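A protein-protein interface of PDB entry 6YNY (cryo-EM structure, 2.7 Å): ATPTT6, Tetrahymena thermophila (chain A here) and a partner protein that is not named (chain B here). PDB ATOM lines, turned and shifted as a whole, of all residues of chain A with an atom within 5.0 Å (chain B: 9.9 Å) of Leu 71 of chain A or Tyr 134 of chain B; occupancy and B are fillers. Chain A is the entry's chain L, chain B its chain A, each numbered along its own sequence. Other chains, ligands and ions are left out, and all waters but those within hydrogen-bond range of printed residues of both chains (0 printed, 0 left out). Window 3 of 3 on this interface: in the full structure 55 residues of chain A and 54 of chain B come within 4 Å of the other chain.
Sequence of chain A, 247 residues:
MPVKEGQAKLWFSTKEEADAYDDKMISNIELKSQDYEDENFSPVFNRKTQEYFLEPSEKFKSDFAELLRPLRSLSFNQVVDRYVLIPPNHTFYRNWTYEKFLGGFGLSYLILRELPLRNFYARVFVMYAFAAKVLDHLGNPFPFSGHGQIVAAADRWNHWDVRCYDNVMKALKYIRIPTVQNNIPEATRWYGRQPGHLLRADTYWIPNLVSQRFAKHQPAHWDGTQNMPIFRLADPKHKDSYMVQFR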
ATOM      1  N   LEU A  68       2.263   6.033  25.397  1.00  0.00           N
ATOM      2  CA  LEU A  68       1.068   5.206  25.467  1.00  0.00           C
ATOM      3  C   LEU A  68       1.345   3.809  25.998  1.00  0.00           C
ATOM      4  O   LEU A  68       0.497   2.924  25.855  1.00  0.00           O
ATOM      5  CB  LEU A  68       0.422   5.111  24.088  1.00  0.00           C
ATOM      6  CG  LEU A  68       0.129   6.441  23.402  1.00  0.00           C
ATOM      7  CD1 LEU A  68      -0.474   6.193  22.045  1.00  0.00           C
ATOM      8  CD2 LEU A  68      -0.792   7.297  24.239  1.00  0.00           C
ATOM      9  N   ARG A  69       2.505   3.590  26.607  1.00  0.00           N
ATOM     10  CA  ARG A  69       2.823   2.266  27.135  1.00  0.00           C
ATOM     11  C   ARG A  69       1.812   1.801  28.171  1.00  0.00           C
ATOM     12  O   ARG A  69       1.303   0.674  28.046  1.00  0.00           O
ATOM     13  CB  ARG A  69       4.242   2.279  27.709  1.00  0.00           C
ATOM     14  CG  ARG A  69       4.683   0.962  28.308  1.00  0.00           C
ATOM     15  CD  ARG A  69       6.106   1.042  28.820  1.00  0.00           C
ATOM     16  NE  ARG A  69       7.063   1.261  27.741  1.00  0.00           N
ATOM     17  CZ  ARG A  69       7.610   0.294  27.011  1.00  0.00           C
ATOM     18  NH1 ARG A  69       7.300  -0.977  27.232  1.00  0.00           N
ATOM     19  NH2 ARG A  69       8.473   0.601  26.053  1.00  0.00           N
ATOM     20  N   PRO A  70       1.477   2.584  29.201  1.00  0.00           N
ATOM     21  CA  PRO A  70       0.519   2.104  30.208  1.00  0.00           C
ATOM     22  C   PRO A  70      -0.890   1.904  29.683  1.00  0.00           C
ATOM     23  O   PRO A  70      -1.723   1.348  30.410  1.00  0.00           O
ATOM     24  CB  PRO A  70       0.556   3.203  31.275  1.00  0.00           C
ATOM     25  CG  PRO A  70       1.059   4.396  30.574  1.00  0.00           C
ATOM     26  CD  PRO A  70       2.008   3.912  29.545  1.00  0.00           C
ATOM     27  N   LEU A  71      -1.189   2.332  28.459  1.00  0.00           N
ATOM     28  CA  LEU A  71      -2.520   2.156  27.899  1.00  0.00           C
ATOM     29  C   LEU A  71      -2.658   0.892  27.066  1.00  0.00           C
ATOM     30  O   LEU A  71      -3.782   0.416  26.873  1.00  0.00           O
ATOM     31  CB  LEU A  71      -2.893   3.358  27.032  1.00  0.00           C
ATOM     32  CG  LEU A  71      -3.064   4.692  27.748  1.00  0.00           C
ATOM     33  CD1 LEU A  71      -3.451   5.753  26.754  1.00  0.00           C
ATOM     34  CD2 LEU A  71      -4.098   4.597  28.849  1.00  0.00           C
ATOM     35  N   ARG A  72      -1.553   0.339  26.568  1.00  0.00           N
ATOM     36  CA  ARG A  72      -1.633  -0.856  25.739  1.00  0.00           C
ATOM     37  C   ARG A  72      -1.907  -2.104  26.563  1.00  0.00           C
ATOM     38  O   ARG A  72      -2.558  -3.033  26.073  1.00  0.00           O
ATOM     39  CB  ARG A  72      -0.344  -1.023  24.940  1.00  0.00           C
ATOM     40  CG  ARG A  72      -0.090   0.114  23.980  1.00  0.00           C
ATOM     41  CD  ARG A  72       0.950  -0.245  22.947  1.00  0.00           C
ATOM     42  NE  ARG A  72       1.093   0.814  21.954  1.00  0.00           N
ATOM     43  CZ  ARG A  72       1.923   1.845  22.069  1.00  0.00           C
ATOM     44  NH1 ARG A  72       2.699   1.972  23.137  1.00  0.00           N
ATOM     45  NH2 ARG A  72       1.976   2.756  21.110  1.00  0.00           N
ATOM     46  N   SER A  73      -1.429  -2.146  27.801  1.00  0.00           N
ATOM     47  CA  SER A  73      -1.683  -3.282  28.673  1.00  0.00           C
ATOM     48  C   SER A  73      -3.080  -3.266  29.270  1.00  0.00           C
ATOM     49  O   SER A  73      -3.480  -4.254  29.896  1.00  0.00           O
ATOM     50  CB  SER A  73      -0.658  -3.309  29.805  1.00  0.00           C
ATOM     51  OG  SER A  73      -0.753  -2.141  30.599  1.00  0.00           O
ATOM     52  N   LEU A  74      -3.829  -2.184  29.092  1.00  0.00           N
ATOM     53  CA  LEU A  74      -5.134  -2.015  29.703  1.00  0.00           C
ATOM     54  C   LEU A  74      -6.230  -1.994  28.649  1.00  0.00           C
ATOM     55  O   LEU A  74      -5.996  -1.698  27.474  1.00  0.00           O
ATOM     56  CB  LEU A  74      -5.188  -0.720  30.513  1.00  0.00           C
ATOM     57  CG  LEU A  74      -4.170  -0.579  31.637  1.00  0.00           C
ATOM     58  CD1 LEU A  74      -4.299   0.788  32.251  1.00  0.00           C
ATOM     59  CD2 LEU A  74      -4.363  -1.654  32.680  1.00  0.00           C
ATOM     60  N   PHE A  76     -10.194  -0.458  27.617  1.00  0.00           N
ATOM     61  CA  PHE A  76     -10.818   0.856  27.709  1.00  0.00           C
ATOM     62  C   PHE A  76     -11.526   1.035  29.044  1.00  0.00           C
ATOM     63  O   PHE A  76     -11.454   2.107  29.653  1.00  0.00           O
ATOM     64  CB  PHE A  76     -11.788   1.052  26.550  1.00  0.00           C
ATOM     65  CG  PHE A  76     -12.405   2.411  26.507  1.00  0.00           C
ATOM     66  CD1 PHE A  76     -11.679   3.498  26.069  1.00  0.00           C
ATOM     67  CD2 PHE A  76     -13.712   2.605  26.900  1.00  0.00           C
ATOM     68  CE1 PHE A  76     -12.241   4.747  26.030  1.00  0.00           C
ATOM     69  CE2 PHE A  76     -14.277   3.851  26.859  1.00  0.00           C
ATOM     70  CZ  PHE A  76     -13.542   4.923  26.424  1.00  0.00           C
ATOM     71  N   VAL A  79      -8.921   1.714  31.570  1.00  0.00           N
ATOM     72  CA  VAL A  79      -8.364   3.053  31.423  1.00  0.00           C
ATOM     73  C   VAL A  79      -9.288   4.086  32.046  1.00  0.00           C
ATOM     74  O   VAL A  79      -8.839   4.998  32.751  1.00  0.00           O
ATOM     75  CB  VAL A  79      -8.105   3.347  29.937  1.00  0.00           C
ATOM     76  CG1 VAL A  79      -7.743   4.799  29.732  1.00  0.00           C
ATOM     77  CG2 VAL A  79      -7.012   2.451  29.411  1.00  0.00           C
ATOM     78  N   TYR A  83      -7.857   6.327  35.129  1.00  0.00           N
ATOM     79  CA  TYR A  83      -7.445   7.714  34.982  1.00  0.00           C
ATOM     80  C   TYR A  83      -8.602   8.697  34.886  1.00  0.00           C
ATOM     81  O   TYR A  83      -8.384   9.898  35.074  1.00  0.00           O
ATOM     82  CB  TYR A  83      -6.566   7.875  33.739  1.00  0.00           C
ATOM     83  CG  TYR A  83      -5.390   6.937  33.700  1.00  0.00           C
ATOM     84  CD1 TYR A  83      -4.344   7.075  34.592  1.00  0.00           C
ATOM     85  CD2 TYR A  83      -5.320   5.919  32.766  1.00  0.00           C
ATOM     86  CE1 TYR A  83      -3.269   6.228  34.562  1.00  0.00           C
ATOM     87  CE2 TYR A  83      -4.246   5.062  32.729  1.00  0.00           C
ATOM     88  CZ  TYR A  83      -3.221   5.223  33.629  1.00  0.00           C
ATOM     89  OH  TYR A  83      -2.142   4.375  33.601  1.00  0.00           O
ATOM     90  N   MET B  78      -2.772  14.960  24.399  1.00  0.00           N
ATOM     91  CA  MET B  78      -2.230  13.692  23.928  1.00  0.00           C
ATOM     92  C   MET B  78      -2.819  13.301  22.580  1.00  0.00           C
ATOM     93  O   MET B  78      -2.121  12.735  21.731  1.00  0.00           O
ATOM     94  CB  MET B  78      -2.489  12.603  24.967  1.00  0.00           C
ATOM     95  CG  MET B  78      -1.979  11.233  24.583  1.00  0.00           C
ATOM     96  SD  MET B  78      -0.213  11.187  24.241  1.00  0.00           S
ATOM     97  CE  MET B  78       0.430  11.543  25.865  1.00  0.00           C
ATOM     98  N   PHE B  79      -4.102  13.590  22.366  1.00  0.00           N
ATOM     99  CA  PHE B  79      -4.734  13.255  21.094  1.00  0.00           C
ATOM    100  C   PHE B  79      -4.111  14.038  19.948  1.00  0.00           C
ATOM    101  O   PHE B  79      -3.732  13.463  18.921  1.00  0.00           O
ATOM    102  CB  PHE B  79      -6.234  13.530  21.171  1.00  0.00           C
ATOM    103  CG  PHE B  79      -6.912  13.541  19.839  1.00  0.00           C
ATOM    104  CD1 PHE B  79      -7.269  12.361  19.223  1.00  0.00           C
ATOM    105  CD2 PHE B  79      -7.191  14.732  19.200  1.00  0.00           C
ATOM    106  CE1 PHE B  79      -7.890  12.370  18.001  1.00  0.00           C
ATOM    107  CE2 PHE B  79      -7.810  14.742  17.976  1.00  0.00           C
ATOM    108  CZ  PHE B  79      -8.160  13.560  17.376  1.00  0.00           C
ATOM    109  N   GLN B  82      -0.580  12.829  19.128  1.00  0.00           N
ATOM    110  CA  GLN B  82      -0.490  11.469  18.613  1.00  0.00           C
ATOM    111  C   GLN B  82      -1.026  11.377  17.192  1.00  0.00           C
ATOM    112  O   GLN B  82      -0.377  10.802  16.312  1.00  0.00           O
ATOM    113  CB  GLN B  82      -1.249  10.513  19.527  1.00  0.00           C
ATOM    114  CG  GLN B  82      -0.534  10.204  20.814  1.00  0.00           C
ATOM    115  CD  GLN B  82       0.725   9.401  20.598  1.00  0.00           C
ATOM    116  OE1 GLN B  82       0.983   8.909  19.501  1.00  0.00           O
ATOM    117  NE2 GLN B  82       1.520   9.266  21.644  1.00  0.00           N
ATOM    118  N   TYR B  83      -2.214  11.928  16.952  1.00  0.00           N
ATOM    119  CA  TYR B  83      -2.783  11.902  15.613  1.00  0.00           C
ATOM    120  C   TYR B  83      -2.061  12.842  14.663  1.00  0.00           C
ATOM    121  O   TYR B  83      -2.130  12.644  13.447  1.00  0.00           O
ATOM    122  CB  TYR B  83      -4.266  12.253  15.667  1.00  0.00           C
ATOM    123  CG  TYR B  83      -5.164  11.053  15.807  1.00  0.00           C
ATOM    124  CD1 TYR B  83      -6.020  10.683  14.786  1.00  0.00           C
ATOM    125  CD2 TYR B  83      -5.142  10.280  16.951  1.00  0.00           C
ATOM    126  CE1 TYR B  83      -6.836   9.587  14.907  1.00  0.00           C
ATOM    127  CE2 TYR B  83      -5.953   9.183  17.082  1.00  0.00           C
ATOM    128  CZ  TYR B  83      -6.799   8.838  16.057  1.00  0.00           C
ATOM    129  OH  TYR B  83      -7.611   7.738  16.188  1.00  0.00           O
ATOM    130  N   ILE B 100      -9.772  14.827  10.783  1.00  0.00           N
ATOM    131  CA  ILE B 100     -10.088  14.624  12.193  1.00  0.00           C
ATOM    132  C   ILE B 100      -9.483  15.733  13.042  1.00  0.00           C
ATOM    133  O   ILE B 100     -10.147  16.308  13.911  1.00  0.00           O
ATOM    134  CB  ILE B 100      -9.600  13.240  12.649  1.00  0.00           C
ATOM    135  CG1 ILE B 100     -10.407  12.141  11.970  1.00  0.00           C
ATOM    136  CG2 ILE B 100      -9.677  13.120  14.146  1.00  0.00           C
ATOM    137  CD1 ILE B 100     -11.862  12.144  12.313  1.00  0.00           C
ATOM    138  N   LEU B 123     -15.232  15.040  26.876  1.00  0.00           N
ATOM    139  CA  LEU B 123     -14.432  15.374  25.704  1.00  0.00           C
ATOM    140  C   LEU B 123     -14.116  16.859  25.610  1.00  0.00           C
ATOM    141  O   LEU B 123     -13.766  17.355  24.536  1.00  0.00           O
ATOM    142  CB  LEU B 123     -15.115  14.896  24.420  1.00  0.00           C
ATOM    143  CG  LEU B 123     -15.177  13.376  24.291  1.00  0.00           C
ATOM    144  CD1 LEU B 123     -16.028  12.964  23.117  1.00  0.00           C
ATOM    145  CD2 LEU B 123     -13.790  12.804  24.164  1.00  0.00           C
ATOM    146  N   GLU B 127     -10.070  15.574  32.337  1.00  0.00           N
ATOM    147  CA  GLU B 127     -10.281  14.186  32.730  1.00  0.00           C
ATOM    148  C   GLU B 127     -10.461  13.291  31.512  1.00  0.00           C
ATOM    149  O   GLU B 127      -9.879  12.204  31.432  1.00  0.00           O
ATOM    150  CB  GLU B 127     -11.507  14.072  33.633  1.00  0.00           C
ATOM    151  CG  GLU B 127     -11.485  14.930  34.868  1.00  0.00           C
ATOM    152  CD  GLU B 127     -12.046  16.314  34.630  1.00  0.00           C
ATOM    153  OE1 GLU B 127     -11.472  17.057  33.809  1.00  0.00           O
ATOM    154  OE2 GLU B 127     -13.071  16.655  35.255  1.00  0.00           O
ATOM    155  N   THR B 128     -11.269  13.736  30.553  1.00  0.00           N
ATOM    156  CA  THR B 128     -11.658  12.933  29.404  1.00  0.00           C
ATOM    157  C   THR B 128     -10.814  13.229  28.173  1.00  0.00           C
ATOM    158  O   THR B 128     -11.284  13.068  27.043  1.00  0.00           O
ATOM    159  CB  THR B 128     -13.134  13.164  29.092  1.00  0.00           C
ATOM    160  OG1 THR B 128     -13.316  14.497  28.603  1.00  0.00           O
ATOM    161  CG2 THR B 128     -13.957  12.993  30.342  1.00  0.00           C
ATOM    162  N   ALA B 129      -9.569  13.656  28.370  1.00  0.00           N
ATOM    163  CA  ALA B 129      -8.709  13.949  27.234  1.00  0.00           C
ATOM    164  C   ALA B 129      -8.211  12.677  26.561  1.00  0.00           C
ATOM    165  O   ALA B 129      -7.921  12.689  25.359  1.00  0.00           O
ATOM    166  CB  ALA B 129      -7.534  14.807  27.685  1.00  0.00           C
ATOM    167  N   LEU B 130      -8.109  11.579  27.307  1.00  0.00           N
ATOM    168  CA  LEU B 130      -7.627  10.329  26.740  1.00  0.00           C
ATOM    169  C   LEU B 130      -8.667   9.630  25.881  1.00  0.00           C
ATOM    170  O   LEU B 130      -8.297   8.857  24.992  1.00  0.00           O
ATOM    171  CB  LEU B 130      -7.183   9.385  27.855  1.00  0.00           C
ATOM    172  CG  LEU B 130      -6.057   9.890  28.752  1.00  0.00           C
ATOM    173  CD1 LEU B 130      -5.822   8.919  29.884  1.00  0.00           C
ATOM    174  CD2 LEU B 130      -4.786  10.092  27.959  1.00  0.00           C
ATOM    175  N   ILE B 131      -9.954   9.882  26.121  1.00  0.00           N
ATOM    176  CA  ILE B 131     -10.998   9.210  25.364  1.00  0.00           C
ATOM    177  C   ILE B 131     -10.947   9.595  23.896  1.00  0.00           C
ATOM    178  O   ILE B 131     -11.428   8.845  23.041  1.00  0.00           O
ATOM    179  CB  ILE B 131     -12.371   9.519  25.991  1.00  0.00           C
ATOM    180  CG1 ILE B 131     -12.443   8.895  27.383  1.00  0.00           C
ATOM    181  CG2 ILE B 131     -13.489   9.008  25.110  1.00  0.00           C
ATOM    182  CD1 ILE B 131     -13.646   9.288  28.175  1.00  0.00           C
ATOM    183  N   TRP B 132     -10.368  10.751  23.579  1.00  0.00           N
ATOM    184  CA  TRP B 132     -10.164  11.117  22.185  1.00  0.00           C
ATOM    185  C   TRP B 132      -9.304  10.095  21.461  1.00  0.00           C
ATOM    186  O   TRP B 132      -9.434   9.924  20.243  1.00  0.00           O
ATOM    187  CB  TRP B 132      -9.512  12.490  22.095  1.00  0.00           C
ATOM    188  CG  TRP B 132     -10.452  13.624  22.252  1.00  0.00           C
ATOM    189  CD1 TRP B 132     -10.653  14.371  23.368  1.00  0.00           C
ATOM    190  CD2 TRP B 132     -11.324  14.152  21.252  1.00  0.00           C
ATOM    191  NE1 TRP B 132     -11.596  15.334  23.129  1.00  0.00           N
ATOM    192  CE2 TRP B 132     -12.026  15.220  21.835  1.00  0.00           C
ATOM    193  CE3 TRP B 132     -11.582  13.824  19.920  1.00  0.00           C
ATOM    194  CZ2 TRP B 132     -12.966  15.960  21.134  1.00  0.00           C
ATOM    195  CZ3 TRP B 132     -12.514  14.561  19.228  1.00  0.00           C
ATOM    196  CH2 TRP B 132     -13.196  15.616  19.834  1.00  0.00           C
ATOM    197  N   LEU B 133      -8.414   9.418  22.183  1.00  0.00           N
ATOM    198  CA  LEU B 133      -7.530   8.446  21.560  1.00  0.00           C
ATOM    199  C   LEU B 133      -8.281   7.212  21.089  1.00  0.00           C
ATOM    200  O   LEU B 133      -7.812   6.527  20.175  1.00  0.00           O
ATOM    201  CB  LEU B 133      -6.438   8.040  22.543  1.00  0.00           C
ATOM    202  CG  LEU B 133      -5.563   9.168  23.076  1.00  0.00           C
ATOM    203  CD1 LEU B 133      -4.694   8.657  24.191  1.00  0.00           C
ATOM    204  CD2 LEU B 133      -4.718   9.746  21.970  1.00  0.00           C
ATOM    205  N   TYR B 134      -9.428   6.920  21.691  1.00  0.00           N
ATOM    206  CA  TYR B 134     -10.206   5.738  21.360  1.00  0.00           C
ATOM    207  C   TYR B 134     -11.396   6.040  20.465  1.00  0.00           C
ATOM    208  O   TYR B 134     -11.737   5.216  19.613  1.00  0.00           O
ATOM    209  CB  TYR B 134     -10.708   5.069  22.639  1.00  0.00           C
ATOM    210  CG  TYR B 134      -9.615   4.572  23.556  1.00  0.00           C
ATOM    211  CD1 TYR B 134      -8.977   5.431  24.432  1.00  0.00           C
ATOM    212  CD2 TYR B 134      -9.231   3.242  23.554  1.00  0.00           C
ATOM    213  CE1 TYR B 134      -7.985   4.983  25.270  1.00  0.00           C
ATOM    214  CE2 TYR B 134      -8.243   2.786  24.389  1.00  0.00           C
ATOM    215  CZ  TYR B 134      -7.622   3.661  25.246  1.00  0.00           C
ATOM    216  OH  TYR B 134      -6.631   3.211  26.083  1.00  0.00           O
ATOM    217  N   HIS B 135     -12.027   7.198  20.636  1.00  0.00           N
ATOM    218  CA  HIS B 135     -13.256   7.549  19.930  1.00  0.00           C
ATOM    219  C   HIS B 135     -13.149   8.968  19.392  1.00  0.00           C
ATOM    220  O   HIS B 135     -13.802   9.891  19.890  1.00  0.00           O
ATOM    221  CB  HIS B 135     -14.466   7.403  20.852  1.00  0.00           C
ATOM    222  CG  HIS B 135     -14.629   6.029  21.412  1.00  0.00           C
ATOM    223  ND1 HIS B 135     -15.009   4.953  20.642  1.00  0.00           N
ATOM    224  CD2 HIS B 135     -14.467   5.555  22.669  1.00  0.00           C
ATOM    225  CE1 HIS B 135     -15.071   3.875  21.400  1.00  0.00           C
ATOM    226  NE2 HIS B 135     -14.748   4.212  22.634  1.00  0.00           N
ATOM    227  N   PRO B 136     -12.334   9.173  18.357  1.00  0.00           N
ATOM    228  CA  PRO B 136     -12.245  10.491  17.724  1.00  0.00           C
ATOM    229  C   PRO B 136     -13.434  10.836  16.843  1.00  0.00           C
ATOM    230  O   PRO B 136     -13.470  11.939  16.288  1.00  0.00           O
ATOM    231  CB  PRO B 136     -10.963  10.373  16.896  1.00  0.00           C
ATOM    232  CG  PRO B 136     -10.873   8.940  16.563  1.00  0.00           C
ATOM    233  CD  PRO B 136     -11.434   8.196  17.727  1.00  0.00           C
ATOM    234  N   GLU B 137     -14.394   9.927  16.701  1.00  0.00           N
ATOM    235  CA  GLU B 137     -15.564  10.154  15.867  1.00  0.00           C
ATOM    236  C   GLU B 137     -16.602  11.053  16.520  1.00  0.00           C
ATOM    237  O   GLU B 137     -17.543  11.476  15.841  1.00  0.00           O
ATOM    238  CB  GLU B 137     -16.223   8.818  15.510  1.00  0.00           C
ATOM    239  CG  GLU B 137     -16.735   8.011  16.693  1.00  0.00           C
ATOM    240  CD  GLU B 137     -15.683   7.110  17.300  1.00  0.00           C
ATOM    241  OE1 GLU B 137     -16.060   6.166  18.024  1.00  0.00           O
ATOM    242  OE2 GLU B 137     -14.483   7.336  17.049  1.00  0.00           O
ATOM    243  N   LEU B 138     -16.461  11.352  17.804  1.00  0.00           N
ATOM    244  CA  LEU B 138     -17.475  12.081  18.549  1.00  0.00           C
ATOM    245  C   LEU B 138     -17.368  13.590  18.401  1.00  0.00           C
ATOM    246  O   LEU B 138     -18.094  14.311  19.092  1.00  0.00           O
ATOM    247  CB  LEU B 138     -17.396  11.694  20.021  1.00  0.00           C
ATOM    248  CG  LEU B 138     -17.649  10.215  20.291  1.00  0.00           C
ATOM    249  CD1 LEU B 138     -17.357   9.881  21.722  1.00  0.00           C
ATOM    250  CD2 LEU B 138     -19.069   9.852  19.955  1.00  0.00           C
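NE2 of Gln 82 of chain B sits close to SD of Met 78 of chain B, at 3.7 Å.
The side-chain carboxylate of Glu 137 of chain B is in hydrogen-bond range of a ring nitrogen (ND1) of His 135 of chain B, at 3.1 Å.
Among the printed residues, pairs that only touch across the chains: Phe 76 of chain A with Tyr 134 of chain B (3.4 Å), Val 79 of chain A with Tyr 134 of chain B (3.4 Å), Leu 68 of chain A with Gln 82 of chain B (3.6 Å), Leu 71 of chain A with Tyr 134 of chain B (3.9 Å), Phe 76 of chain A with His 135 of chain B (3.9 Å) and Leu 68 of chain A with Met 78 of chain B (3.9 Å).
No residue of chain B comes within 4 Å of Pro 70 of chain A.
Leu 71 of chain A touches one residue of chain B.
No residue of chain B comes within 4 Å of Ser 73 of chain A.
Printed residues of chain B within 4 Å of Val 79 of chain A: Tyr 134 (3.4 Å).
Tyr 134 of chain B touches three residues of chain A.
Printed residues of chain A within 4 Å of His 135 of chain B: Phe 76 (3.9 Å).
The nearest residue of chain B that does not touch Leu 71 of chain A is Leu 133 of chain B (4.1 Å).
The nearest printed residue of chain A that does not touch Tyr 134 of chain B is Leu 74 of chain A (5.1 Å).
The nearest printed residue of chain B that does not touch Val 79 of chain A is Leu 130 of chain B (4.5 Å).
Printed residues of chain B that touch a printed residue of chain A: Met 78, Gln 82, Tyr 134 and His 135.
Hydrophobic or aromatic side chains of chain B that line the printed part of chain A: Met 78, Tyr 134 and His 135.
Along chain B the printed residues that touch a printed residue of chain A span positions 78 to 135.
Of the 10 printed residues of chain A, 4 touch a printed residue of chain B.
Hydrophobic or aromatic side chains of chain A that line the printed part of chain B: Leu 68, Leu 71, Phe 76 and Val 79.
Among the printed residues, 6 pairs touch across the chains.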
